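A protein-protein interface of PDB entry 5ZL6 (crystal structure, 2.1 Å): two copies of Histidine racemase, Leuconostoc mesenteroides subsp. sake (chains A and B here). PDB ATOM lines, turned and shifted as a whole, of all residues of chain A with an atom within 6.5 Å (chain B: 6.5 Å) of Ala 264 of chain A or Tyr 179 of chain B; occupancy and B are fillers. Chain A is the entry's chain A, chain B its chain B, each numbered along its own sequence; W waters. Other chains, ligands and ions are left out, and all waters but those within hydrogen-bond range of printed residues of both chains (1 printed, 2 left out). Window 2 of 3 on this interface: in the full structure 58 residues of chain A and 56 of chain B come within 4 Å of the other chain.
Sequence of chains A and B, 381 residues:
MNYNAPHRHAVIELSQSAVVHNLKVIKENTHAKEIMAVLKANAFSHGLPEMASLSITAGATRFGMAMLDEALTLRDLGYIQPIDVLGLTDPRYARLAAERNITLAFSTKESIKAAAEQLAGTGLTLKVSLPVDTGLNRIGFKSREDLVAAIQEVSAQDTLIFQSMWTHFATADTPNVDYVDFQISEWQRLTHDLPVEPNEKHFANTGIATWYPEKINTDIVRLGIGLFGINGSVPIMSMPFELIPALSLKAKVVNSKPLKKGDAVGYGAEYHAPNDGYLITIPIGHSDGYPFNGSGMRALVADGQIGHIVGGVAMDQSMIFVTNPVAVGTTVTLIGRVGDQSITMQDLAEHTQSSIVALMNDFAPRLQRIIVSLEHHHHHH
No position is printed for both chains.
Of the 10 pairs that touch across the chains among the printed residues, none has its exchanged pair printed and touching as well.
Gly 135 of chain B touches Ala 264 of chain A (O to O, 3.6 Å).
Ala 264 of chain A touches Tyr 179 of chain B.
Val 265 of chain A touches Leu 136 of chain B.
Gly 266 of chain A touches Ala 170 of chain B.
CG2 of Thr 171 of chain B touches C of Gly 268 of chain A, 3.7 Å away.
CB of Ala 269 of chain A touches CG2 of Thr 171 of chain B, 3.8 Å away.
Ala 269 of chain A touches Tyr 179 of chain B (CB to CZ, 3.9 Å).
The backbone carbonyl oxygen (O) of Ala 264 of chain A sits at hydrogen-bond distance from the side-chain amide nitrogen (ND2) of Asn 137 of chain B, at 2.6 Å.
N of Gly 266 of chain A is in hydrogen-bond range of O of Leu 136 of chain B (3.1 Å).
The backbone NH (N) of Gly 268 of chain A is in hydrogen-bond range of the backbone carbonyl oxygen (O) of Ala 170 of chain B (2.6 Å).
The backbone carbonyl oxygen (O) of Gly 135 of chain B lies within hydrogen-bond range of the side-chain hydroxyl (OH) of Tyr 179 of chain B (2.6 Å).
The backbone NH (N) of Tyr 179 of chain B sits at hydrogen-bond distance from the side-chain amide oxygen (OD1) of Asn 176 of chain B, at 3.3 Å.
OG1 of Thr 171 of chain B is in hydrogen-bond range of O of Asn 176 of chain B (3.2 Å).
The backbone NH of Ala 170 of chain B lies within hydrogen-bond range of the side-chain amide oxygen of Gln 183 of chain B (2.8 Å).
The backbone NH of Val 265 of chain A is in hydrogen-bond range of the backbone carbonyl oxygen of Tyr 271 of chain A (2.9 Å).
Water W1 lies within hydrogen-bond range of N of Ala 264 of chain A (2.9 Å) and OH of Tyr 179 of chain B (3.1 Å).
Printed residues of chain B that touch a printed residue of chain A: Gly 135, Leu 136, Asn 137, Ala 170, Thr 171 and Tyr 179.
Hydrophobic or aromatic side chains of chain B that line the printed part of chain A: Leu 136, Ala 170 and Tyr 179.
Among the printed residues, 10 pairs touch across the chains.
Among the printed residues, no Asp or Glu carboxylate lies within 4 Å of a Lys or Arg side-chain nitrogen of the other chain.
Of the printed residues of chain B, Ala 264 of chain A touches Gly 135 (3.6 Å), Asn 137 (2.6 Å) and Tyr 179 (3.4 Å).
Printed residues of chain B within 4 Å of Gly 268 of chain A: Ala 170 (2.6 Å) and Thr 171 (3.7 Å).
Printed residues of chain B within 4 Å of Ala 269 of chain A: Thr 171 and Tyr 179.
Of the printed residues of chain A, Gly 135 of chain B touches Ala 264 (3.6 Å).
Of the printed residues of chain A, Ala 170 of chain B touches Gly 266 and Gly 268.
Val 177 of chain B touches none of the printed residues of chain A.
Of chain A, only Ala 264 and Ala 269 come within 4 Å of Tyr 179 of chain B.
The nearest residue of chain B that does not touch Ala 264 of chain A is Leu 136 of chain B (4.2 Å).
The nearest printed residue of chain A that does not touch Asn 137 of chain B is Val 265 of chain A (4.2 Å).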
ATOM      1  N   LEU A 259      24.438   9.861  -7.056  1.00  0.00           N
ATOM      2  CA  LEU A 259      23.717  11.036  -7.508  1.00  0.00           C
ATOM      3  C   LEU A 259      23.460  10.895  -8.997  1.00  0.00           C
ATOM      4  O   LEU A 259      24.213  10.233  -9.713  1.00  0.00           O
ATOM      5  CB  LEU A 259      24.465  12.329  -7.170  1.00  0.00           C
ATOM      6  CG  LEU A 259      25.538  12.896  -8.088  1.00  0.00           C
ATOM      7  CD1 LEU A 259      25.816  14.335  -7.693  1.00  0.00           C
ATOM      8  CD2 LEU A 259      26.795  12.069  -7.986  1.00  0.00           C
ATOM      9  N   LYS A 260      22.362  11.484  -9.448  1.00  0.00           N
ATOM     10  CA  LYS A 260      21.921  11.301 -10.818  1.00  0.00           C
ATOM     11  C   LYS A 260      22.488  12.384 -11.726  1.00  0.00           C
ATOM     12  O   LYS A 260      22.754  13.505 -11.280  1.00  0.00           O
ATOM     13  CB  LYS A 260      20.391  11.282 -10.880  1.00  0.00           C
ATOM     14  CG  LYS A 260      19.764  12.331 -11.790  1.00  0.00           C
ATOM     15  CD  LYS A 260      18.301  12.004 -12.059  1.00  0.00           C
ATOM     16  CE  LYS A 260      17.944  12.209 -13.527  1.00  0.00           C
ATOM     17  NZ  LYS A 260      17.501  13.601 -13.811  1.00  0.00           N
ATOM     18  N   GLY A 262      22.990  15.421 -13.856  1.00  0.00           N
ATOM     19  CA  GLY A 262      22.337  16.709 -13.736  1.00  0.00           C
ATOM     20  C   GLY A 262      22.196  17.240 -12.319  1.00  0.00           C
ATOM     21  O   GLY A 262      21.941  18.427 -12.142  1.00  0.00           O
ATOM     22  N   ASP A 263      22.348  16.382 -11.311  1.00  0.00           N
ATOM     23  CA  ASP A 263      22.263  16.835  -9.921  1.00  0.00           C
ATOM     24  C   ASP A 263      23.339  17.874  -9.610  1.00  0.00           C
ATOM     25  O   ASP A 263      24.515  17.663  -9.896  1.00  0.00           O
ATOM     26  CB  ASP A 263      22.394  15.664  -8.943  1.00  0.00           C
ATOM     27  CG  ASP A 263      21.181  14.757  -8.945  1.00  0.00           C
ATOM     28  OD1 ASP A 263      20.086  15.216  -9.329  1.00  0.00           O
ATOM     29  OD2 ASP A 263      21.324  13.582  -8.549  1.00  0.00           O
ATOM     30  N   ALA A 264      22.928  18.989  -9.014  1.00  0.00           N
ATOM     31  CA  ALA A 264      23.863  20.042  -8.623  1.00  0.00           C
ATOM     32  C   ALA A 264      24.557  19.729  -7.295  1.00  0.00           C
ATOM     33  O   ALA A 264      23.948  19.176  -6.375  1.00  0.00           O
ATOM     34  CB  ALA A 264      23.141  21.377  -8.535  1.00  0.00           C
ATOM     35  N   VAL A 265      25.836  20.082  -7.208  1.00  0.00           N
ATOM     36  CA  VAL A 265      26.624  19.875  -5.996  1.00  0.00           C
ATOM     37  C   VAL A 265      27.331  21.156  -5.555  1.00  0.00           C
ATOM     38  O   VAL A 265      27.887  21.873  -6.378  1.00  0.00           O
ATOM     39  CB  VAL A 265      27.687  18.778  -6.197  1.00  0.00           C
ATOM     40  CG1 VAL A 265      28.451  18.520  -4.900  1.00  0.00           C
ATOM     41  CG2 VAL A 265      27.039  17.502  -6.694  1.00  0.00           C
ATOM     42  N   GLY A 266      27.300  21.442  -4.255  1.00  0.00           N
ATOM     43  CA  GLY A 266      28.090  22.522  -3.697  1.00  0.00           C
ATOM     44  C   GLY A 266      27.419  23.882  -3.715  1.00  0.00           C
ATOM     45  O   GLY A 266      26.382  24.070  -4.353  1.00  0.00           O
ATOM     46  N   GLY A 268      26.424  27.499  -4.689  1.00  0.00           N
ATOM     47  CA  GLY A 268      26.276  28.079  -6.009  1.00  0.00           C
ATOM     48  C   GLY A 268      25.546  27.158  -6.964  1.00  0.00           C
ATOM     49  O   GLY A 268      25.050  27.605  -7.995  1.00  0.00           O
ATOM     50  N   ALA A 269      25.470  25.873  -6.621  1.00  0.00           N
ATOM     51  CA  ALA A 269      24.839  24.887  -7.498  1.00  0.00           C
ATOM     52  C   ALA A 269      25.360  25.017  -8.925  1.00  0.00           C
ATOM     53  O   ALA A 269      24.580  25.139  -9.873  1.00  0.00           O
ATOM     54  CB  ALA A 269      23.328  25.039  -7.477  1.00  0.00           C
ATOM     55  N   GLU A 270      26.679  24.988  -9.081  1.00  0.00           N
ATOM     56  CA  GLU A 270      27.277  25.227 -10.389  1.00  0.00           C
ATOM     57  C   GLU A 270      27.848  23.963 -11.013  1.00  0.00           C
ATOM     58  O   GLU A 270      27.864  23.832 -12.239  1.00  0.00           O
ATOM     59  CB  GLU A 270      28.355  26.304 -10.288  1.00  0.00           C
ATOM     60  CG  GLU A 270      27.848  27.673 -10.702  1.00  0.00           C
ATOM     61  CD  GLU A 270      28.128  28.749  -9.675  1.00  0.00           C
ATOM     62  OE1 GLU A 270      29.021  28.541  -8.825  1.00  0.00           O
ATOM     63  OE2 GLU A 270      27.452  29.800  -9.721  1.00  0.00           O
ATOM     64  N   TYR A 271      28.315  23.033 -10.187  1.00  0.00           N
ATOM     65  CA  TYR A 271      28.676  21.722 -10.706  1.00  0.00           C
ATOM     66  C   TYR A 271      27.409  20.898 -10.858  1.00  0.00           C
ATOM     67  O   TYR A 271      26.612  20.808  -9.928  1.00  0.00           O
ATOM     68  CB  TYR A 271      29.670  20.999  -9.794  1.00  0.00           C
ATOM     69  CG  TYR A 271      29.985  19.581 -10.242  1.00  0.00           C
ATOM     70  CD1 TYR A 271      30.997  19.332 -11.161  1.00  0.00           C
ATOM     71  CD2 TYR A 271      29.270  18.494  -9.746  1.00  0.00           C
ATOM     72  CE1 TYR A 271      31.288  18.044 -11.575  1.00  0.00           C
ATOM     73  CE2 TYR A 271      29.554  17.199 -10.155  1.00  0.00           C
ATOM     74  CZ  TYR A 271      30.566  16.982 -11.067  1.00  0.00           C
ATOM     75  OH  TYR A 271      30.857  15.701 -11.472  1.00  0.00           O
ATOM     76  N   HIS A 272      27.218  20.315 -12.035  1.00  0.00           N
ATOM     77  CA  HIS A 272      26.147  19.355 -12.237  1.00  0.00           C
ATOM     78  C   HIS A 272      26.761  18.043 -12.698  1.00  0.00           C
ATOM     79  O   HIS A 272      27.561  18.023 -13.629  1.00  0.00           O
ATOM     80  CB  HIS A 272      25.126  19.859 -13.259  1.00  0.00           C
ATOM     81  CG  HIS A 272      24.458  21.141 -12.872  1.00  0.00           C
ATOM     82  ND1 HIS A 272      25.052  22.373 -13.042  1.00  0.00           N
ATOM     83  CD2 HIS A 272      23.239  21.383 -12.333  1.00  0.00           C
ATOM     84  CE1 HIS A 272      24.230  23.318 -12.620  1.00  0.00           C
ATOM     85  NE2 HIS A 272      23.124  22.744 -12.183  1.00  0.00           N
ATOM     86  N   ALA A 273      26.404  16.947 -12.039  1.00  0.00           N
ATOM     87  CA  ALA A 273      26.960  15.651 -12.403  1.00  0.00           C
ATOM     88  C   ALA A 273      26.777  15.429 -13.902  1.00  0.00           C
ATOM     89  O   ALA A 273      25.687  15.627 -14.435  1.00  0.00           O
ATOM     90  CB  ALA A 273      26.308  14.540 -11.599  1.00  0.00           C
ATOM     91  N   THR B 134      18.432  18.683   0.554  1.00  0.00           N
ATOM     92  CA  THR B 134      17.441  19.206  -0.380  1.00  0.00           C
ATOM     93  C   THR B 134      18.077  19.795  -1.641  1.00  0.00           C
ATOM     94  O   THR B 134      17.383  20.384  -2.469  1.00  0.00           O
ATOM     95  CB  THR B 134      16.560  20.286   0.275  1.00  0.00           C
ATOM     96  OG1 THR B 134      17.387  21.345   0.775  1.00  0.00           O
ATOM     97  CG2 THR B 134      15.741  19.692   1.418  1.00  0.00           C
ATOM     98  N   GLY B 135      19.390  19.643  -1.793  1.00  0.00           N
ATOM     99  CA  GLY B 135      20.036  20.067  -3.024  1.00  0.00           C
ATOM    100  C   GLY B 135      21.443  20.625  -2.928  1.00  0.00           C
ATOM    101  O   GLY B 135      22.010  21.035  -3.941  1.00  0.00           O
ATOM    102  N   LEU B 136      22.008  20.658  -1.725  1.00  0.00           N
ATOM    103  CA  LEU B 136      23.406  21.030  -1.559  1.00  0.00           C
ATOM    104  C   LEU B 136      24.255  19.820  -1.900  1.00  0.00           C
ATOM    105  O   LEU B 136      25.351  19.937  -2.446  1.00  0.00           O
ATOM    106  CB  LEU B 136      23.690  21.494  -0.130  1.00  0.00           C
ATOM    107  CG  LEU B 136      24.684  22.633   0.122  1.00  0.00           C
ATOM    108  CD1 LEU B 136      25.424  22.403   1.427  1.00  0.00           C
ATOM    109  CD2 LEU B 136      25.660  22.822  -1.021  1.00  0.00           C
ATOM    110  N   ASN B 137      23.721  18.654  -1.562  1.00  0.00           N
ATOM    111  CA  ASN B 137      24.363  17.371  -1.815  1.00  0.00           C
ATOM    112  C   ASN B 137      25.711  17.203  -1.108  1.00  0.00           C
ATOM    113  O   ASN B 137      26.626  16.586  -1.649  1.00  0.00           O
ATOM    114  CB  ASN B 137      24.509  17.156  -3.325  1.00  0.00           C
ATOM    115  CG  ASN B 137      23.218  16.643  -3.967  1.00  0.00           C
ATOM    116  OD1 ASN B 137      22.603  15.688  -3.480  1.00  0.00           O
ATOM    117  ND2 ASN B 137      22.795  17.288  -5.048  1.00  0.00           N
ATOM    118  N   PHE B 169      21.005  25.572   2.500  1.00  0.00           N
ATOM    119  CA  PHE B 169      20.840  26.060   1.132  1.00  0.00           C
ATOM    120  C   PHE B 169      22.164  26.240   0.397  1.00  0.00           C
ATOM    121  O   PHE B 169      23.184  26.570   1.002  1.00  0.00           O
ATOM    122  CB  PHE B 169      20.081  27.383   1.133  1.00  0.00           C
ATOM    123  CG  PHE B 169      18.628  27.243   1.461  1.00  0.00           C
ATOM    124  CD1 PHE B 169      18.206  27.189   2.780  1.00  0.00           C
ATOM    125  CD2 PHE B 169      17.680  27.168   0.453  1.00  0.00           C
ATOM    126  CE1 PHE B 169      16.866  27.060   3.088  1.00  0.00           C
ATOM    127  CE2 PHE B 169      16.341  27.044   0.754  1.00  0.00           C
ATOM    128  CZ  PHE B 169      15.933  26.988   2.077  1.00  0.00           C
ATOM    129  N   ALA B 170      22.129  26.037  -0.915  1.00  0.00           N
ATOM    130  CA  ALA B 170      23.322  26.142  -1.748  1.00  0.00           C
ATOM    131  C   ALA B 170      23.469  27.505  -2.424  1.00  0.00           C
ATOM    132  O   ALA B 170      24.556  27.859  -2.874  1.00  0.00           O
ATOM    133  CB  ALA B 170      23.317  25.043  -2.806  1.00  0.00           C
ATOM    134  N   THR B 171      22.380  28.261  -2.522  1.00  0.00           N
ATOM    135  CA  THR B 171      22.405  29.482  -3.322  1.00  0.00           C
ATOM    136  C   THR B 171      21.709  30.686  -2.671  1.00  0.00           C
ATOM    137  O   THR B 171      21.468  31.691  -3.333  1.00  0.00           O
ATOM    138  CB  THR B 171      21.761  29.250  -4.721  1.00  0.00           C
ATOM    139  OG1 THR B 171      20.343  29.119  -4.591  1.00  0.00           O
ATOM    140  CG2 THR B 171      22.320  28.006  -5.399  1.00  0.00           C
ATOM    141  N   ASN B 176      20.319  33.476  -7.584  1.00  0.00           N
ATOM    142  CA  ASN B 176      19.626  32.275  -8.043  1.00  0.00           C
ATOM    143  C   ASN B 176      18.486  31.907  -7.102  1.00  0.00           C
ATOM    144  O   ASN B 176      18.499  30.843  -6.478  1.00  0.00           O
ATOM    145  CB  ASN B 176      20.614  31.106  -8.167  1.00  0.00           C
ATOM    146  CG  ASN B 176      20.001  29.860  -8.781  1.00  0.00           C
ATOM    147  OD1 ASN B 176      18.787  29.765  -8.958  1.00  0.00           O
ATOM    148  ND2 ASN B 176      20.848  28.888  -9.100  1.00  0.00           N
ATOM    149  N   VAL B 177      17.511  32.801  -6.970  1.00  0.00           N
ATOM    150  CA  VAL B 177      16.290  32.421  -6.298  1.00  0.00           C
ATOM    151  C   VAL B 177      15.947  31.109  -6.946  1.00  0.00           C
ATOM    152  O   VAL B 177      16.575  30.716  -7.923  1.00  0.00           O
ATOM    153  CB  VAL B 177      15.136  33.419  -6.504  1.00  0.00           C
ATOM    154  CG1 VAL B 177      14.193  33.404  -5.306  1.00  0.00           C
ATOM    155  CG2 VAL B 177      15.666  34.814  -6.768  1.00  0.00           C
ATOM    156  N   ASP B 178      14.960  30.412  -6.429  1.00  0.00           N
ATOM    157  CA  ASP B 178      14.340  29.397  -7.262  1.00  0.00           C
ATOM    158  C   ASP B 178      15.184  28.124  -7.455  1.00  0.00           C
ATOM    159  O   ASP B 178      14.631  27.087  -7.810  1.00  0.00           O
ATOM    160  CB  ASP B 178      13.960  30.037  -8.609  1.00  0.00           C
ATOM    161  CG  ASP B 178      14.827  29.579  -9.751  1.00  0.00           C
ATOM    162  OD1 ASP B 178      15.739  28.761  -9.516  1.00  0.00           O
ATOM    163  OD2 ASP B 178      14.589  30.047 -10.890  1.00  0.00           O
ATOM    164  N   TYR B 179      16.498  28.177  -7.221  1.00  0.00           N
ATOM    165  CA  TYR B 179      17.153  26.960  -6.744  1.00  0.00           C
ATOM    166  C   TYR B 179      16.824  26.943  -5.262  1.00  0.00           C
ATOM    167  O   TYR B 179      16.652  25.885  -4.655  1.00  0.00           O
ATOM    168  CB  TYR B 179      18.669  26.912  -6.978  1.00  0.00           C
ATOM    169  CG  TYR B 179      19.237  25.515  -6.731  1.00  0.00           C
ATOM    170  CD1 TYR B 179      19.246  24.565  -7.745  1.00  0.00           C
ATOM    171  CD2 TYR B 179      19.725  25.139  -5.479  1.00  0.00           C
ATOM    172  CE1 TYR B 179      19.739  23.284  -7.533  1.00  0.00           C
ATOM    173  CE2 TYR B 179      20.224  23.852  -5.258  1.00  0.00           C
ATOM    174  CZ  TYR B 179      20.224  22.932  -6.293  1.00  0.00           C
ATOM    175  OH  TYR B 179      20.709  21.652  -6.109  1.00  0.00           O
ATOM    176  N   VAL B 180      16.723  28.142  -4.694  1.00  0.00           N
ATOM    177  CA  VAL B 180      16.192  28.319  -3.349  1.00  0.00           C
ATOM    178  C   VAL B 180      14.798  27.705  -3.279  1.00  0.00           C
ATOM    179  O   VAL B 180      14.506  26.916  -2.379  1.00  0.00           O
ATOM    180  CB  VAL B 180      16.124  29.811  -2.936  1.00  0.00           C
ATOM    181  CG1 VAL B 180      15.327  29.971  -1.657  1.00  0.00           C
ATOM    182  CG2 VAL B 180      17.520  30.384  -2.771  1.00  0.00           C
ATOM    183  N   ASP B 181      13.944  28.065  -4.239  1.00  0.00           N
ATOM    184  CA  ASP B 181      12.593  27.517  -4.314  1.00  0.00           C
ATOM    185  C   ASP B 181      12.643  26.021  -4.572  1.00  0.00           C
ATOM    186  O   ASP B 181      11.785  25.270  -4.104  1.00  0.00           O
ATOM    187  CB  ASP B 181      11.767  28.192  -5.418  1.00  0.00           C
ATOM    188  CG  ASP B 181      11.587  29.685  -5.195  1.00  0.00           C
ATOM    189  OD1 ASP B 181      11.644  30.130  -4.027  1.00  0.00           O
ATOM    190  OD2 ASP B 181      11.378  30.411  -6.192  1.00  0.00           O
ATOM    191  N   PHE B 182      13.638  25.592  -5.341  1.00  0.00           N
ATOM    192  CA  PHE B 182      13.806  24.177  -5.621  1.00  0.00           C
ATOM    193  C   PHE B 182      14.024  23.418  -4.318  1.00  0.00           C
ATOM    194  O   PHE B 182      13.308  22.459  -4.020  1.00  0.00           O
ATOM    195  CB  PHE B 182      14.972  23.942  -6.584  1.00  0.00           C
ATOM    196  CG  PHE B 182      15.361  22.497  -6.722  1.00  0.00           C
ATOM    197  CD1 PHE B 182      14.521  21.597  -7.362  1.00  0.00           C
ATOM    198  CD2 PHE B 182      16.565  22.038  -6.210  1.00  0.00           C
ATOM    199  CE1 PHE B 182      14.873  20.265  -7.488  1.00  0.00           C
ATOM    200  CE2 PHE B 182      16.928  20.710  -6.335  1.00  0.00           C
ATOM    201  CZ  PHE B 182      16.078  19.820  -6.974  1.00  0.00           C
ATOM    202  N   GLN B 183      14.999  23.863  -3.530  1.00  0.00           N
ATOM    203  CA  GLN B 183      15.312  23.190  -2.273  1.00  0.00           C
ATOM    204  C   GLN B 183      14.102  23.157  -1.346  1.00  0.00           C
ATOM    205  O   GLN B 183      13.906  22.196  -0.608  1.00  0.00           O
ATOM    206  CB  GLN B 183      16.500  23.863  -1.580  1.00  0.00           C
ATOM    207  CG  GLN B 183      17.836  23.562  -2.247  1.00  0.00           C
ATOM    208  CD  GLN B 183      19.026  24.064  -1.449  1.00  0.00           C
ATOM    209  OE1 GLN B 183      19.697  25.015  -1.846  1.00  0.00           O
ATOM    210  NE2 GLN B 183      19.295  23.419  -0.320  1.00  0.00           N
ATOM    211  N   ILE B 184      13.279  24.198  -1.402  1.00  0.00           N
ATOM    212  CA  ILE B 184      12.131  24.308  -0.509  1.00  0.00           C
ATOM    213  C   ILE B 184      11.013  23.340  -0.897  1.00  0.00           C
ATOM    214  O   ILE B 184      10.362  22.762  -0.026  1.00  0.00           O
ATOM    215  CB  ILE B 184      11.597  25.750  -0.480  1.00  0.00           C
ATOM    216  CG1 ILE B 184      12.590  26.647   0.266  1.00  0.00           C
ATOM    217  CG2 ILE B 184      10.229  25.801   0.173  1.00  0.00           C
ATOM    218  CD1 ILE B 184      12.336  28.127   0.115  1.00  0.00           C
HETATM  219  O   HOH W   1      20.204  19.368  -8.104  1.00  0.00           O
